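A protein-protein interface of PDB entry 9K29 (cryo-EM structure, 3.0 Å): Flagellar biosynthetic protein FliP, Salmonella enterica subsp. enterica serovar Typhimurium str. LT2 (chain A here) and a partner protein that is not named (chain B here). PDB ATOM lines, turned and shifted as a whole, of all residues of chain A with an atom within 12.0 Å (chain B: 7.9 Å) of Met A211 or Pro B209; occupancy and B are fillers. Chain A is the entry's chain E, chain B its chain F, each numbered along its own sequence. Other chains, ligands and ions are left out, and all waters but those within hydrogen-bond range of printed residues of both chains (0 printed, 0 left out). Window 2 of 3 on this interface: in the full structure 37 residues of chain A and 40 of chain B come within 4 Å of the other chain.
Printed residues of chain B within 4 Å of Met A210: Asn B205 (3.9 Å). Of chain B, only Asn B205, Pro B209, Leu B211, Ser B212 and Ile B213 come within 4 Å of Met A211. Pro A214 touches none of the printed residues of chain B. Of the printed residues of chain A, Gly B202 touches Met A209 (3.6 Å) and Val A212 (3.8 Å). Of the printed residues of chain A, Arg B206 touches Leu A207. No residue of chain A comes within 4 Å of Ala B208. Leu B211 touches one residue of chain A. Of chain A, only Met A211 comes within 4 Å of Ser B212. Of chain A, only Met A211 and Pro A213 come within 4 Å of Ile B213. Val B215 touches none of the printed residues of chain A. The nearest residue of chain B that does not touch Met A211 is Phe B214 (5.8 Å).
Arg B206 touches Leu A207. Gly B202 touches Met A209. Met A210 touches Asn B205. Met A211 touches Pro B209 (CG to O, 3.8 Å). CG of Met A211 touches O of Leu B211, at 3.7 Å. Met A211 touches Ile B213. Val A212 touches Gly B202 (CG2 to CA, 3.8 Å). CZ of Phe B110 touches CB of Pro A213 (3.7 Å). Ile B213 touches Pro A213.
The backbone NH (N) of Met A211 sits close to the side-chain amide nitrogen (ND2) of Asn B205, 3.3 Å away. The side-chain sulfur of Met A211 lies within hydrogen-bond range of the side-chain hydroxyl of Ser B212 (3.8 Å).
Hydrophobic or aromatic side chains of chain B within 4 Å of the printed part of chain A: Phe B110 and Ile B213. Of the 18 printed residues of chain A, 6 touch a printed residue of chain B. Printed residues of chain A that touch a printed residue of chain B: Leu A207, Met A209, Met A210, Met A211, Val A212 and Pro A213. Hydrophobic or aromatic side chains of chain A that line the printed part of chain B: Met A209, Met A211, Val A212 and Pro A213. Among the printed residues, no Asp or Glu carboxylate lies within 4 Å of a Lys or Arg side-chain nitrogen of the other chain.
The backbone carbonyl oxygen of Leu B211 sits close to the side-chain amide oxygen of Asn B205, 3.5 Å away. The side-chain amide oxygen (OD1) of Asn B205 sits close to the backbone carbonyl oxygen (O) of Ala B208 (3.3 Å). O of Ile B213 lies within hydrogen-bond range of N of Phe B218. O of Pro A213 is in hydrogen-bond range of OG1 of Thr A216, at 2.9 Å. The backbone carbonyl oxygen of Gln B210 sits at hydrogen-bond distance from the side-chain hydroxyl of Ser B212 (3.3 Å). The backbone carbonyl oxygen of Leu A204 is in hydrogen-bond range of the backbone NH of Met A209 (3.0 Å).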
ATOM      1  N   ILE A 200      -8.099   7.874  31.784  1.00  0.00           N
ATOM      2  CA  ILE A 200      -9.088   7.350  30.844  1.00  0.00           C
ATOM      3  C   ILE A 200     -10.418   7.110  31.546  1.00  0.00           C
ATOM      4  O   ILE A 200     -11.485   7.468  31.029  1.00  0.00           O
ATOM      5  CB  ILE A 200      -8.564   6.070  30.169  1.00  0.00           C
ATOM      6  CG1 ILE A 200      -7.334   6.384  29.318  1.00  0.00           C
ATOM      7  CG2 ILE A 200      -9.649   5.434  29.317  1.00  0.00           C
ATOM      8  CD1 ILE A 200      -7.608   7.353  28.192  1.00  0.00           C
ATOM      9  N   ALA A 201     -10.379   6.504  32.735  1.00  0.00           N
ATOM     10  CA  ALA A 201     -11.611   6.223  33.463  1.00  0.00           C
ATOM     11  C   ALA A 201     -12.328   7.507  33.858  1.00  0.00           C
ATOM     12  O   ALA A 201     -13.556   7.599  33.751  1.00  0.00           O
ATOM     13  CB  ALA A 201     -11.306   5.372  34.692  1.00  0.00           C
ATOM     14  N   SER A 202     -11.579   8.513  34.317  1.00  0.00           N
ATOM     15  CA  SER A 202     -12.189   9.784  34.691  1.00  0.00           C
ATOM     16  C   SER A 202     -12.795  10.482  33.483  1.00  0.00           C
ATOM     17  O   SER A 202     -13.879  11.066  33.581  1.00  0.00           O
ATOM     18  CB  SER A 202     -11.157  10.681  35.369  1.00  0.00           C
ATOM     19  OG  SER A 202     -10.687  10.096  36.570  1.00  0.00           O
ATOM     20  N   VAL A 203     -12.109  10.444  32.338  1.00  0.00           N
ATOM     21  CA  VAL A 203     -12.654  11.052  31.129  1.00  0.00           C
ATOM     22  C   VAL A 203     -13.944  10.354  30.720  1.00  0.00           C
ATOM     23  O   VAL A 203     -14.932  11.005  30.360  1.00  0.00           O
ATOM     24  CB  VAL A 203     -11.608  11.026  29.998  1.00  0.00           C
ATOM     25  CG1 VAL A 203     -12.272  11.253  28.650  1.00  0.00           C
ATOM     26  CG2 VAL A 203     -10.538  12.075  30.247  1.00  0.00           C
ATOM     27  N   LEU A 204     -13.961   9.021  30.779  1.00  0.00           N
ATOM     28  CA  LEU A 204     -15.179   8.289  30.444  1.00  0.00           C
ATOM     29  C   LEU A 204     -16.311   8.624  31.405  1.00  0.00           C
ATOM     30  O   LEU A 204     -17.461   8.795  30.987  1.00  0.00           O
ATOM     31  CB  LEU A 204     -14.908   6.786  30.445  1.00  0.00           C
ATOM     32  CG  LEU A 204     -14.076   6.244  29.284  1.00  0.00           C
ATOM     33  CD1 LEU A 204     -13.679   4.803  29.544  1.00  0.00           C
ATOM     34  CD2 LEU A 204     -14.847   6.365  27.980  1.00  0.00           C
ATOM     35  N   MET A 205     -16.006   8.729  32.700  1.00  0.00           N
ATOM     36  CA  MET A 205     -17.060   8.913  33.690  1.00  0.00           C
ATOM     37  C   MET A 205     -17.606  10.336  33.664  1.00  0.00           C
ATOM     38  O   MET A 205     -18.802  10.553  33.890  1.00  0.00           O
ATOM     39  CB  MET A 205     -16.536   8.559  35.079  1.00  0.00           C
ATOM     40  CG  MET A 205     -17.589   8.598  36.161  1.00  0.00           C
ATOM     41  SD  MET A 205     -18.858   7.362  35.857  1.00  0.00           S
ATOM     42  CE  MET A 205     -17.960   5.865  36.247  1.00  0.00           C
ATOM     43  N   ALA A 206     -16.745  11.321  33.395  1.00  0.00           N
ATOM     44  CA  ALA A 206     -17.196  12.703  33.299  1.00  0.00           C
ATOM     45  C   ALA A 206     -18.173  12.910  32.153  1.00  0.00           C
ATOM     46  O   ALA A 206     -19.042  13.783  32.245  1.00  0.00           O
ATOM     47  CB  ALA A 206     -15.999  13.639  33.136  1.00  0.00           C
ATOM     48  N   LEU A 207     -18.052  12.130  31.083  1.00  0.00           N
ATOM     49  CA  LEU A 207     -18.967  12.196  29.955  1.00  0.00           C
ATOM     50  C   LEU A 207     -20.143  11.237  30.075  1.00  0.00           C
ATOM     51  O   LEU A 207     -20.683  10.814  29.053  1.00  0.00           O
ATOM     52  CB  LEU A 207     -18.215  11.962  28.644  1.00  0.00           C
ATOM     53  CG  LEU A 207     -17.175  13.011  28.253  1.00  0.00           C
ATOM     54  CD1 LEU A 207     -16.410  12.573  27.015  1.00  0.00           C
ATOM     55  CD2 LEU A 207     -17.837  14.361  28.028  1.00  0.00           C
ATOM     56  N   GLY A 208     -20.523  10.858  31.290  1.00  0.00           N
ATOM     57  CA  GLY A 208     -21.721  10.058  31.496  1.00  0.00           C
ATOM     58  C   GLY A 208     -21.632   8.644  30.965  1.00  0.00           C
ATOM     59  O   GLY A 208     -22.666   7.987  30.790  1.00  0.00           O
ATOM     60  N   MET A 209     -20.421   8.153  30.706  1.00  0.00           N
ATOM     61  CA  MET A 209     -20.250   6.795  30.209  1.00  0.00           C
ATOM     62  C   MET A 209     -19.956   5.844  31.363  1.00  0.00           C
ATOM     63  O   MET A 209     -18.854   5.295  31.458  1.00  0.00           O
ATOM     64  CB  MET A 209     -19.131   6.741  29.169  1.00  0.00           C
ATOM     65  CG  MET A 209     -19.481   7.418  27.854  1.00  0.00           C
ATOM     66  SD  MET A 209     -18.222   7.182  26.587  1.00  0.00           S
ATOM     67  CE  MET A 209     -18.470   8.650  25.592  1.00  0.00           C
ATOM     68  N   MET A 210     -20.936   5.653  32.248  1.00  0.00           N
ATOM     69  CA  MET A 210     -20.713   4.820  33.425  1.00  0.00           C
ATOM     70  C   MET A 210     -20.537   3.355  33.051  1.00  0.00           C
ATOM     71  O   MET A 210     -19.632   2.684  33.557  1.00  0.00           O
ATOM     72  CB  MET A 210     -21.872   4.978  34.406  1.00  0.00           C
ATOM     73  CG  MET A 210     -22.075   6.392  34.895  1.00  0.00           C
ATOM     74  SD  MET A 210     -23.782   6.687  35.372  1.00  0.00           S
ATOM     75  CE  MET A 210     -24.095   5.244  36.386  1.00  0.00           C
ATOM     76  N   MET A 211     -21.390   2.841  32.162  1.00  0.00           N
ATOM     77  CA  MET A 211     -21.417   1.408  31.900  1.00  0.00           C
ATOM     78  C   MET A 211     -20.173   0.919  31.172  1.00  0.00           C
ATOM     79  O   MET A 211     -19.846  -0.269  31.263  1.00  0.00           O
ATOM     80  CB  MET A 211     -22.659   1.049  31.084  1.00  0.00           C
ATOM     81  CG  MET A 211     -23.985   1.281  31.797  1.00  0.00           C
ATOM     82  SD  MET A 211     -24.203   0.308  33.296  1.00  0.00           S
ATOM     83  CE  MET A 211     -23.867   1.539  34.551  1.00  0.00           C
ATOM     84  N   VAL A 212     -19.474   1.796  30.467  1.00  0.00           N
ATOM     85  CA  VAL A 212     -18.350   1.376  29.627  1.00  0.00           C
ATOM     86  C   VAL A 212     -17.156   1.051  30.522  1.00  0.00           C
ATOM     87  O   VAL A 212     -16.729   1.913  31.305  1.00  0.00           O
ATOM     88  CB  VAL A 212     -18.002   2.464  28.618  1.00  0.00           C
ATOM     89  CG1 VAL A 212     -16.986   1.952  27.616  1.00  0.00           C
ATOM     90  CG2 VAL A 212     -19.256   2.947  27.909  1.00  0.00           C
ATOM     91  N   PRO A 213     -16.599  -0.153  30.442  1.00  0.00           N
ATOM     92  CA  PRO A 213     -15.431  -0.489  31.260  1.00  0.00           C
ATOM     93  C   PRO A 213     -14.197   0.242  30.767  1.00  0.00           C
ATOM     94  O   PRO A 213     -13.844   0.161  29.581  1.00  0.00           O
ATOM     95  CB  PRO A 213     -15.294  -2.008  31.077  1.00  0.00           C
ATOM     96  CG  PRO A 213     -15.919  -2.284  29.762  1.00  0.00           C
ATOM     97  CD  PRO A 213     -17.014  -1.270  29.575  1.00  0.00           C
ATOM     98  N   PRO A 214     -13.515   0.978  31.649  1.00  0.00           N
ATOM     99  CA  PRO A 214     -12.350   1.758  31.206  1.00  0.00           C
ATOM    100  C   PRO A 214     -11.161   0.913  30.784  1.00  0.00           C
ATOM    101  O   PRO A 214     -10.286   1.427  30.077  1.00  0.00           O
ATOM    102  CB  PRO A 214     -12.014   2.612  32.435  1.00  0.00           C
ATOM    103  CG  PRO A 214     -12.518   1.811  33.585  1.00  0.00           C
ATOM    104  CD  PRO A 214     -13.758   1.116  33.094  1.00  0.00           C
ATOM    105  N   ALA A 215     -11.094  -0.355  31.196  1.00  0.00           N
ATOM    106  CA  ALA A 215      -9.927  -1.175  30.880  1.00  0.00           C
ATOM    107  C   ALA A 215      -9.796  -1.408  29.381  1.00  0.00           C
ATOM    108  O   ALA A 215      -8.686  -1.362  28.832  1.00  0.00           O
ATOM    109  CB  ALA A 215     -10.007  -2.506  31.626  1.00  0.00           C
ATOM    110  N   THR A 216     -10.917  -1.662  28.701  1.00  0.00           N
ATOM    111  CA  THR A 216     -10.869  -1.956  27.272  1.00  0.00           C
ATOM    112  C   THR A 216     -10.335  -0.771  26.478  1.00  0.00           C
ATOM    113  O   THR A 216      -9.548  -0.946  25.542  1.00  0.00           O
ATOM    114  CB  THR A 216     -12.255  -2.353  26.770  1.00  0.00           C
ATOM    115  OG1 THR A 216     -13.232  -1.442  27.289  1.00  0.00           O
ATOM    116  CG2 THR A 216     -12.599  -3.764  27.220  1.00  0.00           C
ATOM    117  N   ILE A 217     -10.766   0.443  26.821  1.00  0.00           N
ATOM    118  CA  ILE A 217     -10.256   1.629  26.143  1.00  0.00           C
ATOM    119  C   ILE A 217      -8.812   1.903  26.547  1.00  0.00           C
ATOM    120  O   ILE A 217      -7.978   2.268  25.711  1.00  0.00           O
ATOM    121  CB  ILE A 217     -11.163   2.844  26.416  1.00  0.00           C
ATOM    122  CG1 ILE A 217     -12.564   2.617  25.843  1.00  0.00           C
ATOM    123  CG2 ILE A 217     -10.557   4.112  25.836  1.00  0.00           C
ATOM    124  CD1 ILE A 217     -13.523   1.946  26.794  1.00  0.00           C
ATOM    125  N   PHE B 110     -12.356 -11.251  29.466  1.00  0.00           N
ATOM    126  CA  PHE B 110     -12.645 -10.114  30.330  1.00  0.00           C
ATOM    127  C   PHE B 110     -12.398 -10.443  31.795  1.00  0.00           C
ATOM    128  O   PHE B 110     -12.324  -9.532  32.627  1.00  0.00           O
ATOM    129  CB  PHE B 110     -14.085  -9.653  30.126  1.00  0.00           C
ATOM    130  CG  PHE B 110     -14.345  -8.251  30.589  1.00  0.00           C
ATOM    131  CD1 PHE B 110     -13.972  -7.172  29.808  1.00  0.00           C
ATOM    132  CD2 PHE B 110     -14.973  -8.012  31.799  1.00  0.00           C
ATOM    133  CE1 PHE B 110     -14.211  -5.880  30.229  1.00  0.00           C
ATOM    134  CE2 PHE B 110     -15.216  -6.723  32.225  1.00  0.00           C
ATOM    135  CZ  PHE B 110     -14.835  -5.655  31.440  1.00  0.00           C
ATOM    136  N   LEU B 201     -20.420   2.879  21.257  1.00  0.00           N
ATOM    137  CA  LEU B 201     -21.245   2.273  22.298  1.00  0.00           C
ATOM    138  C   LEU B 201     -21.406   3.213  23.486  1.00  0.00           C
ATOM    139  O   LEU B 201     -22.483   3.289  24.086  1.00  0.00           O
ATOM    140  CB  LEU B 201     -20.642   0.941  22.741  1.00  0.00           C
ATOM    141  CG  LEU B 201     -20.597  -0.158  21.679  1.00  0.00           C
ATOM    142  CD1 LEU B 201     -19.617  -1.247  22.080  1.00  0.00           C
ATOM    143  CD2 LEU B 201     -21.983  -0.737  21.446  1.00  0.00           C
ATOM    144  N   GLY B 202     -20.343   3.932  23.845  1.00  0.00           N
ATOM    145  CA  GLY B 202     -20.462   4.936  24.893  1.00  0.00           C
ATOM    146  C   GLY B 202     -21.400   6.068  24.514  1.00  0.00           C
ATOM    147  O   GLY B 202     -22.165   6.563  25.347  1.00  0.00           O
ATOM    148  N   LEU B 204     -23.939   5.740  22.520  1.00  0.00           N
ATOM    149  CA  LEU B 204     -25.258   5.145  22.710  1.00  0.00           C
ATOM    150  C   LEU B 204     -25.655   5.105  24.179  1.00  0.00           C
ATOM    151  O   LEU B 204     -26.827   5.318  24.504  1.00  0.00           O
ATOM    152  CB  LEU B 204     -25.300   3.733  22.123  1.00  0.00           C
ATOM    153  CG  LEU B 204     -25.056   3.610  20.619  1.00  0.00           C
ATOM    154  CD1 LEU B 204     -25.353   2.196  20.145  1.00  0.00           C
ATOM    155  CD2 LEU B 204     -25.891   4.623  19.853  1.00  0.00           C
ATOM    156  N   ASN B 205     -24.700   4.825  25.067  1.00  0.00           N
ATOM    157  CA  ASN B 205     -24.949   4.882  26.502  1.00  0.00           C
ATOM    158  C   ASN B 205     -25.344   6.288  26.940  1.00  0.00           C
ATOM    159  O   ASN B 205     -26.099   6.450  27.906  1.00  0.00           O
ATOM    160  CB  ASN B 205     -23.698   4.423  27.252  1.00  0.00           C
ATOM    161  CG  ASN B 205     -23.944   4.180  28.726  1.00  0.00           C
ATOM    162  OD1 ASN B 205     -25.063   4.314  29.215  1.00  0.00           O
ATOM    163  ND2 ASN B 205     -22.887   3.837  29.448  1.00  0.00           N
ATOM    164  N   ARG B 206     -24.834   7.308  26.247  1.00  0.00           N
ATOM    165  CA  ARG B 206     -25.179   8.691  26.574  1.00  0.00           C
ATOM    166  C   ARG B 206     -26.686   8.913  26.554  1.00  0.00           C
ATOM    167  O   ARG B 206     -27.265   9.411  27.525  1.00  0.00           O
ATOM    168  CB  ARG B 206     -24.501   9.647  25.594  1.00  0.00           C
ATOM    169  CG  ARG B 206     -23.026   9.824  25.813  1.00  0.00           C
ATOM    170  CD  ARG B 206     -22.805  10.604  27.081  1.00  0.00           C
ATOM    171  NE  ARG B 206     -23.495  11.888  27.060  1.00  0.00           N
ATOM    172  CZ  ARG B 206     -22.998  12.996  26.532  1.00  0.00           C
ATOM    173  NH1 ARG B 206     -21.802  13.017  25.966  1.00  0.00           N
ATOM    174  NH2 ARG B 206     -23.718  14.114  26.571  1.00  0.00           N
ATOM    175  N   MET B 207     -27.340   8.545  25.452  1.00  0.00           N
ATOM    176  CA  MET B 207     -28.767   8.824  25.321  1.00  0.00           C
ATOM    177  C   MET B 207     -29.593   7.895  26.200  1.00  0.00           C
ATOM    178  O   MET B 207     -30.701   8.250  26.619  1.00  0.00           O
ATOM    179  CB  MET B 207     -29.194   8.715  23.857  1.00  0.00           C
ATOM    180  CG  MET B 207     -29.064   7.324  23.263  1.00  0.00           C
ATOM    181  SD  MET B 207     -29.484   7.287  21.510  1.00  0.00           S
ATOM    182  CE  MET B 207     -28.052   8.096  20.803  1.00  0.00           C
ATOM    183  N   ALA B 208     -29.075   6.707  26.490  1.00  0.00           N
ATOM    184  CA  ALA B 208     -29.783   5.763  27.342  1.00  0.00           C
ATOM    185  C   ALA B 208     -28.804   5.059  28.272  1.00  0.00           C
ATOM    186  O   ALA B 208     -28.049   4.183  27.833  1.00  0.00           O
ATOM    187  CB  ALA B 208     -30.545   4.742  26.498  1.00  0.00           C
ATOM    188  N   PRO B 209     -28.779   5.417  29.559  1.00  0.00           N
ATOM    189  CA  PRO B 209     -27.935   4.672  30.507  1.00  0.00           C
ATOM    190  C   PRO B 209     -28.346   3.222  30.655  1.00  0.00           C
ATOM    191  O   PRO B 209     -27.546   2.409  31.135  1.00  0.00           O
ATOM    192  CB  PRO B 209     -28.112   5.447  31.820  1.00  0.00           C
ATOM    193  CG  PRO B 209     -29.421   6.148  31.670  1.00  0.00           C
ATOM    194  CD  PRO B 209     -29.526   6.501  30.216  1.00  0.00           C
ATOM    195  N   GLN B 210     -29.574   2.873  30.264  1.00  0.00           N
ATOM    196  CA  GLN B 210     -30.022   1.489  30.352  1.00  0.00           C
ATOM    197  C   GLN B 210     -29.242   0.584  29.409  1.00  0.00           C
ATOM    198  O   GLN B 210     -29.060  -0.603  29.704  1.00  0.00           O
ATOM    199  CB  GLN B 210     -31.515   1.412  30.053  1.00  0.00           C
ATOM    200  CG  GLN B 210     -32.380   2.089  31.094  1.00  0.00           C
ATOM    201  CD  GLN B 210     -33.842   2.004  30.744  1.00  0.00           C
ATOM    202  OE1 GLN B 210     -34.199   1.495  29.685  1.00  0.00           O
ATOM    203  NE2 GLN B 210     -34.700   2.504  31.625  1.00  0.00           N
ATOM    204  N   LEU B 211     -28.794   1.110  28.272  1.00  0.00           N
ATOM    205  CA  LEU B 211     -27.884   0.355  27.422  1.00  0.00           C
ATOM    206  C   LEU B 211     -26.594   0.091  28.184  1.00  0.00           C
ATOM    207  O   LEU B 211     -25.989   1.011  28.742  1.00  0.00           O
ATOM    208  CB  LEU B 211     -27.588   1.112  26.128  1.00  0.00           C
ATOM    209  CG  LEU B 211     -28.741   1.733  25.338  1.00  0.00           C
ATOM    210  CD1 LEU B 211     -28.252   2.204  23.979  1.00  0.00           C
ATOM    211  CD2 LEU B 211     -29.880   0.749  25.173  1.00  0.00           C
ATOM    212  N   SER B 212     -26.172  -1.168  28.208  1.00  0.00           N
ATOM    213  CA  SER B 212     -25.001  -1.572  28.966  1.00  0.00           C
ATOM    214  C   SER B 212     -24.024  -2.276  28.041  1.00  0.00           C
ATOM    215  O   SER B 212     -24.395  -2.783  26.979  1.00  0.00           O
ATOM    216  CB  SER B 212     -25.379  -2.489  30.137  1.00  0.00           C
ATOM    217  OG  SER B 212     -26.281  -1.842  31.016  1.00  0.00           O
ATOM    218  N   ILE B 213     -22.756  -2.288  28.451  1.00  0.00           N
ATOM    219  CA  ILE B 213     -21.740  -2.970  27.659  1.00  0.00           C
ATOM    220  C   ILE B 213     -22.031  -4.466  27.604  1.00  0.00           C
ATOM    221  O   ILE B 213     -21.950  -5.085  26.537  1.00  0.00           O
ATOM    222  CB  ILE B 213     -20.331  -2.659  28.205  1.00  0.00           C
ATOM    223  CG1 ILE B 213     -19.261  -3.170  27.240  1.00  0.00           C
ATOM    224  CG2 ILE B 213     -20.132  -3.214  29.613  1.00  0.00           C
ATOM    225  CD1 ILE B 213     -19.246  -2.449  25.913  1.00  0.00           C
ATOM    226  N   PHE B 214     -22.432  -5.053  28.736  1.00  0.00           N
ATOM    227  CA  PHE B 214     -22.793  -6.467  28.766  1.00  0.00           C
ATOM    228  C   PHE B 214     -23.992  -6.764  27.877  1.00  0.00           C
ATOM    229  O   PHE B 214     -24.000  -7.774  27.162  1.00  0.00           O
ATOM    230  CB  PHE B 214     -23.102  -6.899  30.201  1.00  0.00           C
ATOM    231  CG  PHE B 214     -21.916  -6.862  31.119  1.00  0.00           C
ATOM    232  CD1 PHE B 214     -20.997  -7.896  31.124  1.00  0.00           C
ATOM    233  CD2 PHE B 214     -21.720  -5.794  31.975  1.00  0.00           C
ATOM    234  CE1 PHE B 214     -19.906  -7.866  31.967  1.00  0.00           C
ATOM    235  CE2 PHE B 214     -20.629  -5.758  32.822  1.00  0.00           C
ATOM    236  CZ  PHE B 214     -19.720  -6.795  32.818  1.00  0.00           C
ATOM    237  N   VAL B 215     -25.011  -5.906  27.914  1.00  0.00           N
ATOM    238  CA  VAL B 215     -26.252  -6.175  27.197  1.00  0.00           C
ATOM    239  C   VAL B 215     -26.055  -6.063  25.691  1.00  0.00           C
ATOM    240  O   VAL B 215     -26.552  -6.897  24.926  1.00  0.00           O
ATOM    241  CB  VAL B 215     -27.357  -5.227  27.694  1.00  0.00           C
ATOM    242  CG1 VAL B 215     -28.651  -5.468  26.930  1.00  0.00           C
ATOM    243  CG2 VAL B 215     -27.568  -5.395  29.188  1.00  0.00           C
ATOM    244  N   PHE B 218     -20.903  -6.229  24.036  1.00  0.00           N
ATOM    245  CA  PHE B 218     -20.131  -7.462  23.885  1.00  0.00           C
ATOM    246  C   PHE B 218     -20.557  -8.292  22.679  1.00  0.00           C
ATOM    247  O   PHE B 218     -19.675  -8.707  21.908  1.00  0.00           O
ATOM    248  CB  PHE B 218     -20.181  -8.265  25.187  1.00  0.00           C
ATOM    249  CG  PHE B 218     -19.363  -7.665  26.294  1.00  0.00           C
ATOM    250  CD1 PHE B 218     -18.394  -6.714  26.021  1.00  0.00           C
ATOM    251  CD2 PHE B 218     -19.581  -8.028  27.611  1.00  0.00           C
ATOM    252  CE1 PHE B 218     -17.642  -6.159  27.036  1.00  0.00           C
ATOM    253  CE2 PHE B 218     -18.838  -7.465  28.630  1.00  0.00           C
ATOM    254  CZ  PHE B 218     -17.866  -6.534  28.343  1.00  0.00           C
